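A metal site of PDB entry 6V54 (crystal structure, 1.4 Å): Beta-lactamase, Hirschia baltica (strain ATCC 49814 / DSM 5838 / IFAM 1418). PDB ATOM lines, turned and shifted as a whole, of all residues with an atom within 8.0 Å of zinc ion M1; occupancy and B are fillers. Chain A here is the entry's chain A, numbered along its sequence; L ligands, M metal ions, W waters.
NE2 of His 215 binds zinc ion M1.
Water W1 is bound to zinc ion M1 (2.1 Å).
The side-chain carboxylate (OD2) of Asp 94 binds zinc ion M1.
The side-chain sulfur (SG) of Cys 173 is bound to zinc ion M1.
O1 of the ligand binds zinc ion M1, 2.5 Å away.
N of Cys 173 is in hydrogen-bond range of OG of Ser 214, 3.2 Å away.
O of Arg 44 sits at hydrogen-bond distance from ND1 of His 215, 2.7 Å away.
Along chain A the residues within 4 Å of zinc ion M1 span positions 94 to 215.
The nearest printed residue that does not touch zinc ion M1 is His 154 (4.3 Å).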
ATOM      1  N   ILE A  43       7.485  10.915  19.119  1.00  0.00           N
ATOM      2  CA  ILE A  43       7.344   9.929  18.052  1.00  0.00           C
ATOM      3  C   ILE A  43       8.613   9.998  17.206  1.00  0.00           C
ATOM      4  O   ILE A  43       9.040  11.089  16.807  1.00  0.00           O
ATOM      5  CB  ILE A  43       6.075  10.174  17.218  1.00  0.00           C
ATOM      6  CG1 ILE A  43       6.099   9.358  15.933  1.00  0.00           C
ATOM      7  CG2 ILE A  43       5.864  11.651  16.917  1.00  0.00           C
ATOM      8  CD1 ILE A  43       4.890   8.576  15.673  1.00  0.00           C
ATOM      9  N   ARG A  44       9.239   8.854  16.959  1.00  0.00           N
ATOM     10  CA  ARG A  44      10.422   8.761  16.130  1.00  0.00           C
ATOM     11  C   ARG A  44      10.056   8.752  14.653  1.00  0.00           C
ATOM     12  O   ARG A  44       8.981   8.291  14.263  1.00  0.00           O
ATOM     13  CB  ARG A  44      11.231   7.482  16.435  1.00  0.00           C
ATOM     14  CG  ARG A  44      10.668   6.226  15.842  1.00  0.00           C
ATOM     15  CD  ARG A  44      11.379   5.000  16.357  1.00  0.00           C
ATOM     16  NE  ARG A  44      12.717   4.830  15.806  1.00  0.00           N
ATOM     17  CZ  ARG A  44      13.569   3.905  16.221  1.00  0.00           C
ATOM     18  NH1 ARG A  44      13.232   3.098  17.235  1.00  0.00           N
ATOM     19  NH2 ARG A  44      14.773   3.826  15.675  1.00  0.00           N
ATOM     20  N   THR A  45      10.984   9.212  13.837  1.00  0.00           N
ATOM     21  CA  THR A  45      10.932   8.966  12.409  1.00  0.00           C
ATOM     22  C   THR A  45      12.334   8.567  11.973  1.00  0.00           C
ATOM     23  O   THR A  45      13.318   9.125  12.454  1.00  0.00           O
ATOM     24  CB  THR A  45      10.382  10.161  11.581  1.00  0.00           C
ATOM     25  OG1 THR A  45      10.245   9.728  10.218  1.00  0.00           O
ATOM     26  CG2 THR A  45      11.308  11.396  11.622  1.00  0.00           C
ATOM     27  N   ASN A  46      12.416   7.569  11.106  1.00  0.00           N
ATOM     28  CA  ASN A  46      13.664   7.010  10.638  1.00  0.00           C
ATOM     29  C   ASN A  46      13.852   7.263   9.153  1.00  0.00           C
ATOM     30  O   ASN A  46      12.884   7.175   8.380  1.00  0.00           O
ATOM     31  CB  ASN A  46      13.637   5.487  10.794  1.00  0.00           C
ATOM     32  CG  ASN A  46      13.412   5.032  12.216  1.00  0.00           C
ATOM     33  OD1 ASN A  46      13.868   5.664  13.163  1.00  0.00           O
ATOM     34  ND2 ASN A  46      12.770   3.888  12.353  1.00  0.00           N
ATOM     35  N   TRP A  63      12.298  15.406  11.095  1.00  0.00           N
ATOM     36  CA  TRP A  63      11.074  16.192  11.248  1.00  0.00           C
ATOM     37  C   TRP A  63      11.201  17.662  10.848  1.00  0.00           C
ATOM     38  O   TRP A  63      10.191  18.286  10.492  1.00  0.00           O
ATOM     39  CB  TRP A  63      10.586  16.152  12.694  1.00  0.00           C
ATOM     40  CG  TRP A  63      10.127  14.837  13.182  1.00  0.00           C
ATOM     41  CD1 TRP A  63      10.821  13.970  13.964  1.00  0.00           C
ATOM     42  CD2 TRP A  63       8.832  14.268  12.972  1.00  0.00           C
ATOM     43  NE1 TRP A  63      10.030  12.876  14.278  1.00  0.00           N
ATOM     44  CE2 TRP A  63       8.812  13.032  13.653  1.00  0.00           C
ATOM     45  CE3 TRP A  63       7.705  14.671  12.255  1.00  0.00           C
ATOM     46  CZ2 TRP A  63       7.684  12.222  13.677  1.00  0.00           C
ATOM     47  CZ3 TRP A  63       6.581  13.864  12.270  1.00  0.00           C
ATOM     48  CH2 TRP A  63       6.584  12.642  12.976  1.00  0.00           C
ATOM     49  N   THR A  89      10.341   9.638   0.507  1.00  0.00           N
ATOM     50  CA  THR A  89       9.491   8.484   0.263  1.00  0.00           C
ATOM     51  C   THR A  89       8.002   8.759   0.256  1.00  0.00           C
ATOM     52  O   THR A  89       7.263   7.892  -0.182  1.00  0.00           O
ATOM     53  CB  THR A  89       9.888   7.289   1.151  1.00  0.00           C
ATOM     54  OG1 THR A  89       9.761   7.648   2.539  1.00  0.00           O
ATOM     55  CG2 THR A  89      11.354   6.922   0.863  1.00  0.00           C
ATOM     56  N   HIS A  90       7.542   9.920   0.745  1.00  0.00           N
ATOM     57  CA  HIS A  90       6.192  10.424   0.459  1.00  0.00           C
ATOM     58  C   HIS A  90       6.090  11.822   1.055  1.00  0.00           C
ATOM     59  O   HIS A  90       6.974  12.270   1.799  1.00  0.00           O
ATOM     60  CB  HIS A  90       5.058   9.523   0.981  1.00  0.00           C
ATOM     61  CG  HIS A  90       4.952   9.459   2.466  1.00  0.00           C
ATOM     62  ND1 HIS A  90       5.777   8.661   3.233  1.00  0.00           N
ATOM     63  CD2 HIS A  90       4.083  10.039   3.321  1.00  0.00           C
ATOM     64  CE1 HIS A  90       5.470   8.819   4.510  1.00  0.00           C
ATOM     65  NE2 HIS A  90       4.440   9.660   4.591  1.00  0.00           N
ATOM     66  N   HIS A  92       4.886  13.831   3.506  1.00  0.00           N
ATOM     67  CA  HIS A  92       4.497  14.180   4.873  1.00  0.00           C
ATOM     68  C   HIS A  92       5.695  14.822   5.546  1.00  0.00           C
ATOM     69  O   HIS A  92       6.836  14.646   5.113  1.00  0.00           O
ATOM     70  CB  HIS A  92       4.032  12.942   5.672  1.00  0.00           C
ATOM     71  CG  HIS A  92       2.603  12.536   5.432  1.00  0.00           C
ATOM     72  ND1 HIS A  92       2.108  11.259   5.714  1.00  0.00           N
ATOM     73  CD2 HIS A  92       1.550  13.257   4.986  1.00  0.00           C
ATOM     74  CE1 HIS A  92       0.809  11.227   5.448  1.00  0.00           C
ATOM     75  NE2 HIS A  92       0.448  12.424   5.024  1.00  0.00           N
ATOM     76  N   SER A  93       5.453  15.494   6.665  1.00  0.00           N
ATOM     77  CA  SER A  93       6.499  16.308   7.271  1.00  0.00           C
ATOM     78  C   SER A  93       7.593  15.483   7.973  1.00  0.00           C
ATOM     79  O   SER A  93       8.675  16.007   8.250  1.00  0.00           O
ATOM     80  CB  SER A  93       5.918  17.348   8.213  1.00  0.00           C
ATOM     81  OG  SER A  93       5.405  16.726   9.365  1.00  0.00           O
ATOM     82  N   ASP A  94       7.343  14.230   8.296  1.00  0.00           N
ATOM     83  CA  ASP A  94       8.433  13.404   8.817  1.00  0.00           C
ATOM     84  C   ASP A  94       9.438  13.026   7.741  1.00  0.00           C
ATOM     85  O   ASP A  94      10.569  12.625   8.090  1.00  0.00           O
ATOM     86  CB  ASP A  94       7.946  12.152   9.558  1.00  0.00           C
ATOM     87  CG  ASP A  94       6.902  11.357   8.813  1.00  0.00           C
ATOM     88  OD1 ASP A  94       6.181  11.817   7.922  1.00  0.00           O
ATOM     89  OD2 ASP A  94       6.746  10.214   9.196  1.00  0.00           O
ATOM     90  N   LYS A  95       9.066  13.094   6.463  1.00  0.00           N
ATOM     91  CA  LYS A  95       9.936  12.696   5.371  1.00  0.00           C
ATOM     92  C   LYS A  95      10.469  13.884   4.607  1.00  0.00           C
ATOM     93  O   LYS A  95      11.487  13.756   3.891  1.00  0.00           O
ATOM     94  CB  LYS A  95       9.161  11.800   4.381  1.00  0.00           C
ATOM     95  CG  LYS A  95       8.280  10.676   4.975  1.00  0.00           C
ATOM     96  CD  LYS A  95       9.117   9.460   5.388  1.00  0.00           C
ATOM     97  CE  LYS A  95       9.816   9.561   6.750  1.00  0.00           C
ATOM     98  NZ  LYS A  95      10.748   8.352   6.891  1.00  0.00           N
ATOM     99  N   HIS A 154       0.052   3.859   2.824  1.00  0.00           N
ATOM    100  CA  HIS A 154      -0.035   4.868   3.871  1.00  0.00           C
ATOM    101  C   HIS A 154      -0.319   6.244   3.263  1.00  0.00           C
ATOM    102  O   HIS A 154      -1.044   7.069   3.858  1.00  0.00           O
ATOM    103  CB  HIS A 154       1.339   4.898   4.583  1.00  0.00           C
ATOM    104  CG  HIS A 154       1.582   6.136   5.363  1.00  0.00           C
ATOM    105  ND1 HIS A 154       1.008   6.354   6.592  1.00  0.00           N
ATOM    106  CD2 HIS A 154       2.287   7.258   5.055  1.00  0.00           C
ATOM    107  CE1 HIS A 154       1.373   7.560   7.021  1.00  0.00           C
ATOM    108  NE2 HIS A 154       2.150   8.116   6.115  1.00  0.00           N
ATOM    109  N   GLY A 172       9.695   2.713   4.969  1.00  0.00           N
ATOM    110  CA  GLY A 172       9.138   3.991   5.374  1.00  0.00           C
ATOM    111  C   GLY A 172       7.825   3.815   6.114  1.00  0.00           C
ATOM    112  O   GLY A 172       7.633   2.851   6.883  1.00  0.00           O
ATOM    113  N   CYS A 173       6.892   4.739   5.878  1.00  0.00           N
ATOM    114  CA  CYS A 173       5.689   4.734   6.681  1.00  0.00           C
ATOM    115  C   CYS A 173       4.645   3.747   6.170  1.00  0.00           C
ATOM    116  O   CYS A 173       3.641   3.505   6.873  1.00  0.00           O
ATOM    117  CB  CYS A 173       5.081   6.127   6.717  1.00  0.00           C
ATOM    118  SG  CYS A 173       6.256   7.368   7.368  1.00  0.00           S
ATOM    119  N   MET A 174       4.904   3.145   5.023  1.00  0.00           N
ATOM    120  CA  MET A 174       3.993   2.144   4.497  1.00  0.00           C
ATOM    121  C   MET A 174       4.067   0.873   5.341  1.00  0.00           C
ATOM    122  O   MET A 174       3.143   0.071   5.316  1.00  0.00           O
ATOM    123  CB  MET A 174       4.404   1.802   3.073  1.00  0.00           C
ATOM    124  CG  MET A 174       3.302   1.056   2.297  1.00  0.00           C
ATOM    125  SD  MET A 174       3.843   0.734   0.485  1.00  0.00           S
ATOM    126  CE  MET A 174       4.762  -0.829   0.773  1.00  0.00           C
ATOM    127  N   ILE A 175       5.174   0.683   6.079  1.00  0.00           N
ATOM    128  CA  ILE A 175       5.325  -0.492   6.916  1.00  0.00           C
ATOM    129  C   ILE A 175       5.150  -0.057   8.362  1.00  0.00           C
ATOM    130  O   ILE A 175       5.848   0.852   8.830  1.00  0.00           O
ATOM    131  CB  ILE A 175       6.686  -1.159   6.687  1.00  0.00           C
ATOM    132  CG1 ILE A 175       6.847  -1.532   5.207  1.00  0.00           C
ATOM    133  CG2 ILE A 175       6.832  -2.383   7.552  1.00  0.00           C
ATOM    134  CD1 ILE A 175       5.699  -2.418   4.628  1.00  0.00           C
ATOM    135  N   ARG A 176       4.191  -0.707   9.075  1.00  0.00           N
ATOM    136  CA  ARG A 176       3.921  -0.373  10.464  1.00  0.00           C
ATOM    137  C   ARG A 176       4.908  -1.107  11.385  1.00  0.00           C
ATOM    138  O   ARG A 176       5.423  -2.170  11.026  1.00  0.00           O
ATOM    139  CB  ARG A 176       2.481  -0.774  10.783  1.00  0.00           C
ATOM    140  CG  ARG A 176       1.452   0.028   9.988  1.00  0.00           C
ATOM    141  CD  ARG A 176       1.445   1.514  10.357  1.00  0.00           C
ATOM    142  NE  ARG A 176       1.117   1.702  11.780  1.00  0.00           N
ATOM    143  CZ  ARG A 176       1.617   2.666  12.552  1.00  0.00           C
ATOM    144  NH1 ARG A 176       2.510   3.563  12.098  1.00  0.00           N
ATOM    145  NH2 ARG A 176       1.248   2.700  13.823  1.00  0.00           N
ATOM    146  N   GLY A 184      -1.698   4.042  12.463  1.00  0.00           N
ATOM    147  CA  GLY A 184      -0.948   5.283  12.433  1.00  0.00           C
ATOM    148  C   GLY A 184      -1.800   6.405  11.840  1.00  0.00           C
ATOM    149  O   GLY A 184      -3.040   6.363  11.865  1.00  0.00           O
ATOM    150  N   ASN A 185      -1.111   7.373  11.233  1.00  0.00           N
ATOM    151  CA  ASN A 185      -1.792   8.492  10.587  1.00  0.00           C
ATOM    152  C   ASN A 185      -2.378   8.028   9.265  1.00  0.00           C
ATOM    153  O   ASN A 185      -1.640   7.818   8.308  1.00  0.00           O
ATOM    154  CB  ASN A 185      -0.784   9.627  10.363  1.00  0.00           C
ATOM    155  CG  ASN A 185      -1.351  10.757   9.509  1.00  0.00           C
ATOM    156  OD1 ASN A 185      -2.563  10.824   9.263  1.00  0.00           O
ATOM    157  ND2 ASN A 185      -0.464  11.638   9.036  1.00  0.00           N
ATOM    158  N   PRO A 213      10.870   0.249   9.169  1.00  0.00           N
ATOM    159  CA  PRO A 213       9.689   1.120   9.173  1.00  0.00           C
ATOM    160  C   PRO A 213      10.124   2.516   9.631  1.00  0.00           C
ATOM    161  O   PRO A 213      11.176   2.688  10.263  1.00  0.00           O
ATOM    162  CB  PRO A 213       8.813   0.469  10.256  1.00  0.00           C
ATOM    163  CG  PRO A 213       9.891  -0.027  11.330  1.00  0.00           C
ATOM    164  CD  PRO A 213      11.117  -0.397  10.493  1.00  0.00           C
ATOM    165  N   SER A 214       9.337   3.525   9.290  1.00  0.00           N
ATOM    166  CA  SER A 214       9.689   4.866   9.753  1.00  0.00           C
ATOM    167  C   SER A 214       9.500   5.061  11.235  1.00  0.00           C
ATOM    168  O   SER A 214      10.236   5.861  11.832  1.00  0.00           O
ATOM    169  CB  SER A 214       8.831   5.940   9.109  1.00  0.00           C
ATOM    170  OG  SER A 214       9.117   6.090   7.736  1.00  0.00           O
ATOM    171  N   HIS A 215       8.497   4.419  11.842  1.00  0.00           N
ATOM    172  CA  HIS A 215       8.056   4.795  13.184  1.00  0.00           C
ATOM    173  C   HIS A 215       8.286   3.700  14.223  1.00  0.00           C
ATOM    174  O   HIS A 215       7.581   3.647  15.229  1.00  0.00           O
ATOM    175  CB  HIS A 215       6.607   5.289  13.180  1.00  0.00           C
ATOM    176  CG  HIS A 215       6.403   6.496  12.297  1.00  0.00           C
ATOM    177  ND1 HIS A 215       7.082   7.681  12.490  1.00  0.00           N
ATOM    178  CD2 HIS A 215       5.627   6.672  11.198  1.00  0.00           C
ATOM    179  CE1 HIS A 215       6.722   8.554  11.567  1.00  0.00           C
ATOM    180  NE2 HIS A 215       5.827   7.975  10.768  1.00  0.00           N
HETATM  181  C1  LIG L   1       2.424   7.562  10.092  1.00  0.00           C
HETATM  182  O1  LIG L   1       3.245   7.448   9.276  1.00  0.00           O
HETATM  183  O2  LIG L   1       1.981   6.590  10.620  1.00  0.00           O
HETATM  184 ZN    ZN M   1       5.348   8.684   8.918  1.00  0.00          ZN
HETATM  185 ZN    ZN M   2       3.287   9.761   6.264  1.00  0.00          ZN
HETATM  186  O   HOH W   1       4.076  10.061   8.024  1.00  0.00           O
